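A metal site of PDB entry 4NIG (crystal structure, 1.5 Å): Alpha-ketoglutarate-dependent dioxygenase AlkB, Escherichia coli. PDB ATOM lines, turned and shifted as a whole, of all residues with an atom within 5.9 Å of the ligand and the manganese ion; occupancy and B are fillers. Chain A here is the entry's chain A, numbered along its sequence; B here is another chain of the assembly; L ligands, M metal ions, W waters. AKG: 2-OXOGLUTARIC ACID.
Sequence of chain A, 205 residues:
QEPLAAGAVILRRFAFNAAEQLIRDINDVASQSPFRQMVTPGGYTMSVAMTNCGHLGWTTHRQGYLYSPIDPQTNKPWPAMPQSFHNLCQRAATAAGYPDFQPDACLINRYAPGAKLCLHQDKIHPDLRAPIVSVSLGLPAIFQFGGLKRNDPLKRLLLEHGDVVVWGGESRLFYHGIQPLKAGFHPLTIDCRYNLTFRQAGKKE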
ATOM      1  N   MET A  50      12.780  21.500  17.717  1.00  0.00           N
ATOM      2  CA  MET A  50      12.423  21.937  16.350  1.00  0.00           C
ATOM      3  C   MET A  50      13.447  22.883  15.723  1.00  0.00           C
ATOM      4  O   MET A  50      14.153  23.609  16.426  1.00  0.00           O
ATOM      5  CB  MET A  50      11.081  22.696  16.408  1.00  0.00           C
ATOM      6  CG  MET A  50       9.917  21.827  16.794  1.00  0.00           C
ATOM      7  SD  MET A  50       8.315  22.670  16.994  1.00  0.00           S
ATOM      8  CE  MET A  50       7.258  21.272  16.722  1.00  0.00           C
ATOM      9  N   LEU A 107       9.191  22.354   8.647  1.00  0.00           N
ATOM     10  CA  LEU A 107       9.369  22.284  10.087  1.00  0.00           C
ATOM     11  C   LEU A 107       9.982  20.910  10.324  1.00  0.00           C
ATOM     12  O   LEU A 107       9.458  19.884   9.896  1.00  0.00           O
ATOM     13  CB  LEU A 107       7.989  22.429  10.801  1.00  0.00           C
ATOM     14  CG  LEU A 107       7.975  22.167  12.279  1.00  0.00           C
ATOM     15  CD1 LEU A 107       8.927  23.126  12.993  1.00  0.00           C
ATOM     16  CD2 LEU A 107       6.580  22.282  12.864  1.00  0.00           C
ATOM     17  N   ASN A 109      11.241  18.311  13.144  1.00  0.00           N
ATOM     18  CA  ASN A 109      10.960  17.903  14.519  1.00  0.00           C
ATOM     19  C   ASN A 109      11.987  16.803  14.883  1.00  0.00           C
ATOM     20  O   ASN A 109      12.184  15.884  14.074  1.00  0.00           O
ATOM     21  CB  ASN A 109       9.573  17.299  14.641  1.00  0.00           C
ATOM     22  CG  ASN A 109       8.442  18.331  14.650  1.00  0.00           C
ATOM     23  OD1 ASN A 109       7.288  17.936  14.874  1.00  0.00           O
ATOM     24  ND2 ASN A 109       8.715  19.546  14.426  1.00  0.00           N
ATOM     25  N   TYR A 111      12.408  13.983  17.970  1.00  0.00           N
ATOM     26  CA  TYR A 111      11.848  13.342  19.134  1.00  0.00           C
ATOM     27  C   TYR A 111      12.892  12.469  19.842  1.00  0.00           C
ATOM     28  O   TYR A 111      13.405  11.528  19.229  1.00  0.00           O
ATOM     29  CB  TYR A 111      10.646  12.445  18.751  1.00  0.00           C
ATOM     30  CG  TYR A 111       9.466  13.165  18.098  1.00  0.00           C
ATOM     31  CD1 TYR A 111       9.524  13.579  16.796  1.00  0.00           C
ATOM     32  CD2 TYR A 111       8.320  13.391  18.827  1.00  0.00           C
ATOM     33  CE1 TYR A 111       8.432  14.209  16.194  1.00  0.00           C
ATOM     34  CE2 TYR A 111       7.229  14.045  18.244  1.00  0.00           C
ATOM     35  CZ  TYR A 111       7.314  14.444  16.952  1.00  0.00           C
ATOM     36  OH  TYR A 111       6.258  15.101  16.369  1.00  0.00           O
ATOM     37  N   LEU A 117       3.700  15.089  20.844  1.00  0.00           N
ATOM     38  CA  LEU A 117       3.102  16.277  20.341  1.00  0.00           C
ATOM     39  C   LEU A 117       1.594  16.110  20.475  1.00  0.00           C
ATOM     40  O   LEU A 117       0.989  15.319  19.752  1.00  0.00           O
ATOM     41  CB  LEU A 117       3.487  16.493  18.890  1.00  0.00           C
ATOM     42  CG  LEU A 117       3.347  17.868  18.297  1.00  0.00           C
ATOM     43  CD1 LEU A 117       4.131  18.916  19.071  1.00  0.00           C
ATOM     44  CD2 LEU A 117       3.758  17.832  16.832  1.00  0.00           C
ATOM     45  N   HIS A 120      -3.477  18.516  17.837  1.00  0.00           N
ATOM     46  CA  HIS A 120      -3.535  19.897  17.363  1.00  0.00           C
ATOM     47  C   HIS A 120      -3.973  19.899  15.908  1.00  0.00           C
ATOM     48  O   HIS A 120      -4.017  18.863  15.244  1.00  0.00           O
ATOM     49  CB  HIS A 120      -2.156  20.615  17.508  1.00  0.00           C
ATOM     50  CG  HIS A 120      -1.090  20.064  16.618  1.00  0.00           C
ATOM     51  ND1 HIS A 120      -0.353  18.968  16.976  1.00  0.00           N
ATOM     52  CD2 HIS A 120      -0.660  20.432  15.373  1.00  0.00           C
ATOM     53  CE1 HIS A 120       0.470  18.665  15.983  1.00  0.00           C
ATOM     54  NE2 HIS A 120       0.354  19.564  15.041  1.00  0.00           N
ATOM     55  N   GLN A 121      -4.293  21.100  15.422  1.00  0.00           N
ATOM     56  CA  GLN A 121      -4.579  21.352  14.009  1.00  0.00           C
ATOM     57  C   GLN A 121      -3.448  22.198  13.423  1.00  0.00           C
ATOM     58  O   GLN A 121      -2.941  23.084  14.115  1.00  0.00           O
ATOM     59  CB  GLN A 121      -5.886  22.154  13.875  1.00  0.00           C
ATOM     60  CG  GLN A 121      -7.126  21.464  14.388  1.00  0.00           C
ATOM     61  CD  GLN A 121      -8.345  22.393  14.360  1.00  0.00           C
ATOM     62  OE1 GLN A 121      -8.470  23.341  15.149  1.00  0.00           O
ATOM     63  NE2 GLN A 121      -9.210  22.138  13.427  1.00  0.00           N
ATOM     64  N   ASP A 122      -3.097  21.941  12.164  1.00  0.00           N
ATOM     65  CA  ASP A 122      -2.146  22.810  11.450  1.00  0.00           C
ATOM     66  C   ASP A 122      -3.025  23.893  10.824  1.00  0.00           C
ATOM     67  O   ASP A 122      -3.819  23.602   9.941  1.00  0.00           O
ATOM     68  CB  ASP A 122      -1.350  22.023  10.410  1.00  0.00           C
ATOM     69  CG  ASP A 122      -0.066  21.393  10.979  1.00  0.00           C
ATOM     70  OD1 ASP A 122      -0.157  20.809  12.066  1.00  0.00           O
ATOM     71  OD2 ASP A 122       1.065  21.504  10.332  1.00  0.00           O
ATOM     72  N   ILE A 132      -0.555  19.176   3.488  1.00  0.00           N
ATOM     73  CA  ILE A 132       0.536  18.997   4.409  1.00  0.00           C
ATOM     74  C   ILE A 132       1.211  17.696   4.043  1.00  0.00           C
ATOM     75  O   ILE A 132       0.524  16.683   3.857  1.00  0.00           O
ATOM     76  CB  ILE A 132       0.033  18.899   5.829  1.00  0.00           C
ATOM     77  CG1 ILE A 132      -0.773  20.165   6.167  1.00  0.00           C
ATOM     78  CG2 ILE A 132       1.204  18.679   6.790  1.00  0.00           C
ATOM     79  CD1 ILE A 132      -0.902  20.437   7.623  1.00  0.00           C
ATOM     80  N   SER A 134       4.160  15.070   5.392  1.00  0.00           N
ATOM     81  CA  SER A 134       4.810  14.760   6.672  1.00  0.00           C
ATOM     82  C   SER A 134       5.653  13.481   6.574  1.00  0.00           C
ATOM     83  O   SER A 134       5.149  12.385   6.407  1.00  0.00           O
ATOM     84  CB  SER A 134       3.726  14.502   7.733  1.00  0.00           C
ATOM     85  OG  SER A 134       4.107  14.628   9.075  1.00  0.00           O
ATOM     86  N   SER A 136       8.468  10.749   8.027  1.00  0.00           N
ATOM     87  CA  SER A 136       9.039  10.094   9.237  1.00  0.00           C
ATOM     88  C   SER A 136      10.394   9.491   8.965  1.00  0.00           C
ATOM     89  O   SER A 136      10.561   8.795   7.939  1.00  0.00           O
ATOM     90  CB  SER A 136       8.241   8.912   9.727  1.00  0.00           C
ATOM     91  OG  SER A 136       6.943   9.365  10.112  1.00  0.00           O
ATOM     92  N   PHE A 143       1.090   7.754  15.608  1.00  0.00           N
ATOM     93  CA  PHE A 143       0.478   8.936  15.056  1.00  0.00           C
ATOM     94  C   PHE A 143      -1.015   8.798  15.269  1.00  0.00           C
ATOM     95  O   PHE A 143      -1.592   7.758  14.962  1.00  0.00           O
ATOM     96  CB  PHE A 143       0.743   8.966  13.562  1.00  0.00           C
ATOM     97  CG  PHE A 143       0.205  10.182  12.818  1.00  0.00           C
ATOM     98  CD1 PHE A 143       0.634  11.479  13.100  1.00  0.00           C
ATOM     99  CD2 PHE A 143      -0.674  10.010  11.773  1.00  0.00           C
ATOM    100  CE1 PHE A 143       0.170  12.556  12.378  1.00  0.00           C
ATOM    101  CE2 PHE A 143      -1.152  11.082  11.032  1.00  0.00           C
ATOM    102  CZ  PHE A 143      -0.727  12.349  11.345  1.00  0.00           C
ATOM    103  N   LEU A 159       4.004   4.884  12.592  1.00  0.00           N
ATOM    104  CA  LEU A 159       4.717   5.470  11.478  1.00  0.00           C
ATOM    105  C   LEU A 159       6.164   5.001  11.642  1.00  0.00           C
ATOM    106  O   LEU A 159       6.753   5.201  12.710  1.00  0.00           O
ATOM    107  CB  LEU A 159       4.614   7.002  11.481  1.00  0.00           C
ATOM    108  CG  LEU A 159       3.192   7.626  11.293  1.00  0.00           C
ATOM    109  CD1 LEU A 159       3.315   9.115  11.174  1.00  0.00           C
ATOM    110  CD2 LEU A 159       2.566   7.011  10.076  1.00  0.00           C
ATOM    111  N   TRP A 167      -1.969  15.000   4.021  1.00  0.00           N
ATOM    112  CA  TRP A 167      -3.396  15.356   4.200  1.00  0.00           C
ATOM    113  C   TRP A 167      -3.711  16.697   3.600  1.00  0.00           C
ATOM    114  O   TRP A 167      -2.861  17.545   3.398  1.00  0.00           O
ATOM    115  CB  TRP A 167      -3.882  15.182   5.651  1.00  0.00           C
ATOM    116  CG  TRP A 167      -3.260  15.986   6.764  1.00  0.00           C
ATOM    117  CD1 TRP A 167      -3.819  17.055   7.414  1.00  0.00           C
ATOM    118  CD2 TRP A 167      -2.030  15.705   7.465  1.00  0.00           C
ATOM    119  NE1 TRP A 167      -3.043  17.483   8.434  1.00  0.00           N
ATOM    120  CE2 TRP A 167      -1.911  16.691   8.480  1.00  0.00           C
ATOM    121  CE3 TRP A 167      -1.002  14.757   7.306  1.00  0.00           C
ATOM    122  CZ2 TRP A 167      -0.822  16.725   9.355  1.00  0.00           C
ATOM    123  CZ3 TRP A 167       0.083  14.805   8.172  1.00  0.00           C
ATOM    124  CH2 TRP A 167       0.161  15.777   9.177  1.00  0.00           C
ATOM    125  N   HIS A 176      -4.434  16.033  14.881  1.00  0.00           N
ATOM    126  CA  HIS A 176      -3.488  14.950  14.796  1.00  0.00           C
ATOM    127  C   HIS A 176      -2.398  15.203  15.836  1.00  0.00           C
ATOM    128  O   HIS A 176      -2.269  16.314  16.347  1.00  0.00           O
ATOM    129  CB  HIS A 176      -2.849  14.876  13.399  1.00  0.00           C
ATOM    130  CG  HIS A 176      -2.183  16.152  13.008  1.00  0.00           C
ATOM    131  ND1 HIS A 176      -2.876  17.245  12.550  1.00  0.00           N
ATOM    132  CD2 HIS A 176      -0.883  16.524  13.033  1.00  0.00           C
ATOM    133  CE1 HIS A 176      -2.060  18.246  12.354  1.00  0.00           C
ATOM    134  NE2 HIS A 176      -0.834  17.828  12.609  1.00  0.00           N
ATOM    135  N   GLY A 177      -1.594  14.171  16.112  1.00  0.00           N
ATOM    136  CA  GLY A 177      -0.525  14.254  17.107  1.00  0.00           C
ATOM    137  C   GLY A 177       0.303  13.010  17.137  1.00  0.00           C
ATOM    138  O   GLY A 177       0.045  12.061  16.394  1.00  0.00           O
ATOM    139  N   ILE A 178       1.298  13.015  18.025  1.00  0.00           N
ATOM    140  CA  ILE A 178       2.251  11.880  18.221  1.00  0.00           C
ATOM    141  C   ILE A 178       2.258  11.506  19.711  1.00  0.00           C
ATOM    142  O   ILE A 178       2.374  12.354  20.579  1.00  0.00           O
ATOM    143  CB  ILE A 178       3.662  12.291  17.743  1.00  0.00           C
ATOM    144  CG1 ILE A 178       3.652  12.530  16.227  1.00  0.00           C
ATOM    145  CG2 ILE A 178       4.759  11.281  18.175  1.00  0.00           C
ATOM    146  CD1 ILE A 178       3.646  11.287  15.367  1.00  0.00           C
ATOM    147  N   ARG A 193      13.704  10.025  16.632  1.00  0.00           N
ATOM    148  CA  ARG A 193      12.930  10.120  15.419  1.00  0.00           C
ATOM    149  C   ARG A 193      12.959  11.579  14.942  1.00  0.00           C
ATOM    150  O   ARG A 193      12.977  12.521  15.748  1.00  0.00           O
ATOM    151  CB  ARG A 193      11.469   9.719  15.718  1.00  0.00           C
ATOM    152  CG  ARG A 193      10.411  10.091  14.671  1.00  0.00           C
ATOM    153  CD  ARG A 193       9.027   9.515  14.994  1.00  0.00           C
ATOM    154  NE  ARG A 193       8.122   9.681  13.860  1.00  0.00           N
ATOM    155  CZ  ARG A 193       7.310  10.719  13.675  1.00  0.00           C
ATOM    156  NH1 ARG A 193       7.213  11.680  14.592  1.00  0.00           N
ATOM    157  NH2 ARG A 193       6.541  10.736  12.573  1.00  0.00           N
ATOM    158  N   ASN A 195      10.958  14.182  12.091  1.00  0.00           N
ATOM    159  CA  ASN A 195       9.850  14.392  11.139  1.00  0.00           C
ATOM    160  C   ASN A 195      10.024  15.675  10.345  1.00  0.00           C
ATOM    161  O   ASN A 195      10.442  16.670  10.885  1.00  0.00           O
ATOM    162  CB  ASN A 195       8.535  14.403  11.896  1.00  0.00           C
ATOM    163  CG  ASN A 195       7.346  14.328  10.973  1.00  0.00           C
ATOM    164  OD1 ASN A 195       6.734  15.339  10.695  1.00  0.00           O
ATOM    165  ND2 ASN A 195       7.055  13.144  10.476  1.00  0.00           N
ATOM    166  N   THR A 197       7.821  18.347   8.155  1.00  0.00           N
ATOM    167  CA  THR A 197       6.457  18.824   7.830  1.00  0.00           C
ATOM    168  C   THR A 197       6.590  19.964   6.829  1.00  0.00           C
ATOM    169  O   THR A 197       7.110  21.045   7.146  1.00  0.00           O
ATOM    170  CB  THR A 197       5.819  19.266   9.117  1.00  0.00           C
ATOM    171  OG1 THR A 197       5.631  18.151  10.028  1.00  0.00           O
ATOM    172  CG2 THR A 197       4.464  19.804   8.771  1.00  0.00           C
ATOM    173  P   6MA B   8      -2.565  23.334  20.726  1.00  0.00           P
ATOM    174  OP1 6MA B   8      -2.213  24.655  20.108  1.00  0.00           O
ATOM    175  OP2 6MA B   8      -3.338  22.349  19.970  1.00  0.00           O
ATOM    176  O5' 6MA B   8      -1.080  22.613  21.006  1.00  0.00           O
ATOM    177  C5' 6MA B   8      -0.980  21.227  21.299  1.00  0.00           C
ATOM    178  C4' 6MA B   8       0.490  20.867  20.979  1.00  0.00           C
ATOM    179  O4' 6MA B   8       0.654  20.984  19.554  1.00  0.00           O
ATOM    180  C3' 6MA B   8       1.432  21.785  21.675  1.00  0.00           C
ATOM    181  O3' 6MA B   8       2.679  21.085  21.917  1.00  0.00           O
ATOM    182  C2' 6MA B   8       1.883  22.757  20.594  1.00  0.00           C
ATOM    183  C1' 6MA B   8       1.741  21.943  19.296  1.00  0.00           C
ATOM    184  N9  6MA B   8       1.337  22.703  18.082  1.00  0.00           N
ATOM    185  C8  6MA B   8       0.195  23.453  17.957  1.00  0.00           C
ATOM    186  N7  6MA B   8       0.032  23.939  16.707  1.00  0.00           N
ATOM    187  C5  6MA B   8       1.088  23.455  15.985  1.00  0.00           C
ATOM    188  C6  6MA B   8       1.502  23.578  14.586  1.00  0.00           C
ATOM    189  N1  6MA B   8       2.622  22.914  14.238  1.00  0.00           N
ATOM    190  C2  6MA B   8       3.326  22.123  15.110  1.00  0.00           C
ATOM    191  N3  6MA B   8       2.981  21.983  16.408  1.00  0.00           N
ATOM    192  C4  6MA B   8       1.880  22.618  16.876  1.00  0.00           C
ATOM    193  N6  6MA B   8       0.746  24.375  13.755  1.00  0.00           N
ATOM    194  C1  6MA B   8       1.244  24.636  12.392  1.00  0.00           C
HETATM  195  C1  AKG L   1       3.876  18.898  13.253  1.00  0.00           C
HETATM  196  O1  AKG L   1       5.105  19.198  13.390  1.00  0.00           O
HETATM  197  O2  AKG L   1       3.025  19.774  12.982  1.00  0.00           O
HETATM  198  C2  AKG L   1       3.402  17.537  13.393  1.00  0.00           C
HETATM  199  O5  AKG L   1       2.219  17.323  13.503  1.00  0.00           O
HETATM  200  C3  AKG L   1       4.384  16.392  13.379  1.00  0.00           C
HETATM  201  C4  AKG L   1       3.764  15.010  13.332  1.00  0.00           C
HETATM  202  C5  AKG L   1       4.844  13.924  13.265  1.00  0.00           C
HETATM  203  O3  AKG L   1       5.911  14.110  13.897  1.00  0.00           O
HETATM  204  O4  AKG L   1       4.568  12.919  12.604  1.00  0.00           O
HETATM  205 MN    MN M   1       0.903  19.210  12.893  1.00  0.00          MN
HETATM  206  O   HOH W   1       7.759  18.253  11.629  1.00  0.00           O
HETATM  207  O   HOH W   2       3.280  17.019  10.366  1.00  0.00           O
HETATM  208  O   HOH W   3       3.142  12.521  10.371  1.00  0.00           O
HETATM  209  O   HOH W   4       1.367  18.736  10.598  1.00  0.00           O
HETATM  210  O   HOH W   5       3.230  22.087  11.680  1.00  0.00           O
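An oxygen (O1) of the ligand lies close to the side-chain amide oxygen of Asn 109. NH1 of Arg 193 is in salt-bridge range of O3 of the ligand. ND2 of Asn 195 is in hydrogen-bond range of O4 of the ligand (3.3 Å). The side-chain hydroxyl (OH) of Tyr 111 is in hydrogen-bond range of an oxygen (O3) of the ligand (2.7 Å).
The side-chain amide oxygen of Asn 109 sits at hydrogen-bond distance from the side-chain hydroxyl of Tyr 111 (3.4 Å). The backbone carbonyl oxygen (O) of Leu 117 sits at hydrogen-bond distance from the backbone NH (N) of Ile 178 (2.9 Å). The backbone carbonyl oxygen (O) of Leu 107 sits at hydrogen-bond distance from the backbone NH (N) of Thr 197, at 2.8 Å. The side-chain hydroxyl (OG1) of Thr 197 sits at hydrogen-bond distance from the side-chain amide oxygen (OD1) of Asn 195 (3.1 Å). The backbone carbonyl oxygen (O) of Arg 193 sits at hydrogen-bond distance from the backbone NH (N) of Tyr 111 (2.7 Å). OD1 of Asn 195 lies within hydrogen-bond range of OG of Ser 134, 3.2 Å away. The side-chain amide nitrogen (ND2) of Asn 195 lies close to the guanidinium group (NH2) of Arg 193 (3.2 Å). O of Asn 109 sits at hydrogen-bond distance from N of Asn 195 (2.9 Å).
N1 of 6MA 8 of chain B lies close to an oxygen (O2) of the ligand. Residues that only touch the ligand: Ile 178 (3.3 Å), Leu 107 (3.5 Å), Leu 117 (3.5 Å), Thr 197 (3.6 Å) and Ser 134 (3.9 Å). Hydrophobic or aromatic side chains that line the ligand: Leu 107, Tyr 111, Leu 117, His 120, His 176 and Ile 178.
The nearest printed residue that does not touch the manganese ion is 6MA 8 of chain B (4.3 Å).
The side-chain carboxylate (OD1) of Asp 122 binds the manganese ion, at 2.1 Å. O2 of the ligand is bound to the manganese ion (2.2 Å). A ring nitrogen (NE2) of His 176 binds the manganese ion (2.2 Å). The manganese ion is bound by NE2 of His 120 (2.2 Å). The manganese ion is bound by O5 of the ligand, 2.4 Å away. Water W4 is bound to the manganese ion (2.4 Å). The manganese ion has six donor atoms within binding distance.
Water W5 bridges OD2 of Asp 122 (2.6 Å) and N1 of 6MA 8 of chain B (2.8 Å). Water W3 lies within hydrogen-bond range of OG of Ser 134 and O4 of the ligand. Water W2 bridges OG1 of Thr 197 and OG of Ser 134. Water W1 lies within hydrogen-bond range of OG1 of Thr 197 (2.7 Å), O of Leu 107 (2.9 Å), O of Asn 195 (3.2 Å), ND2 of Asn 109 (3.2 Å) and O1 of the ligand (3.3 Å).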
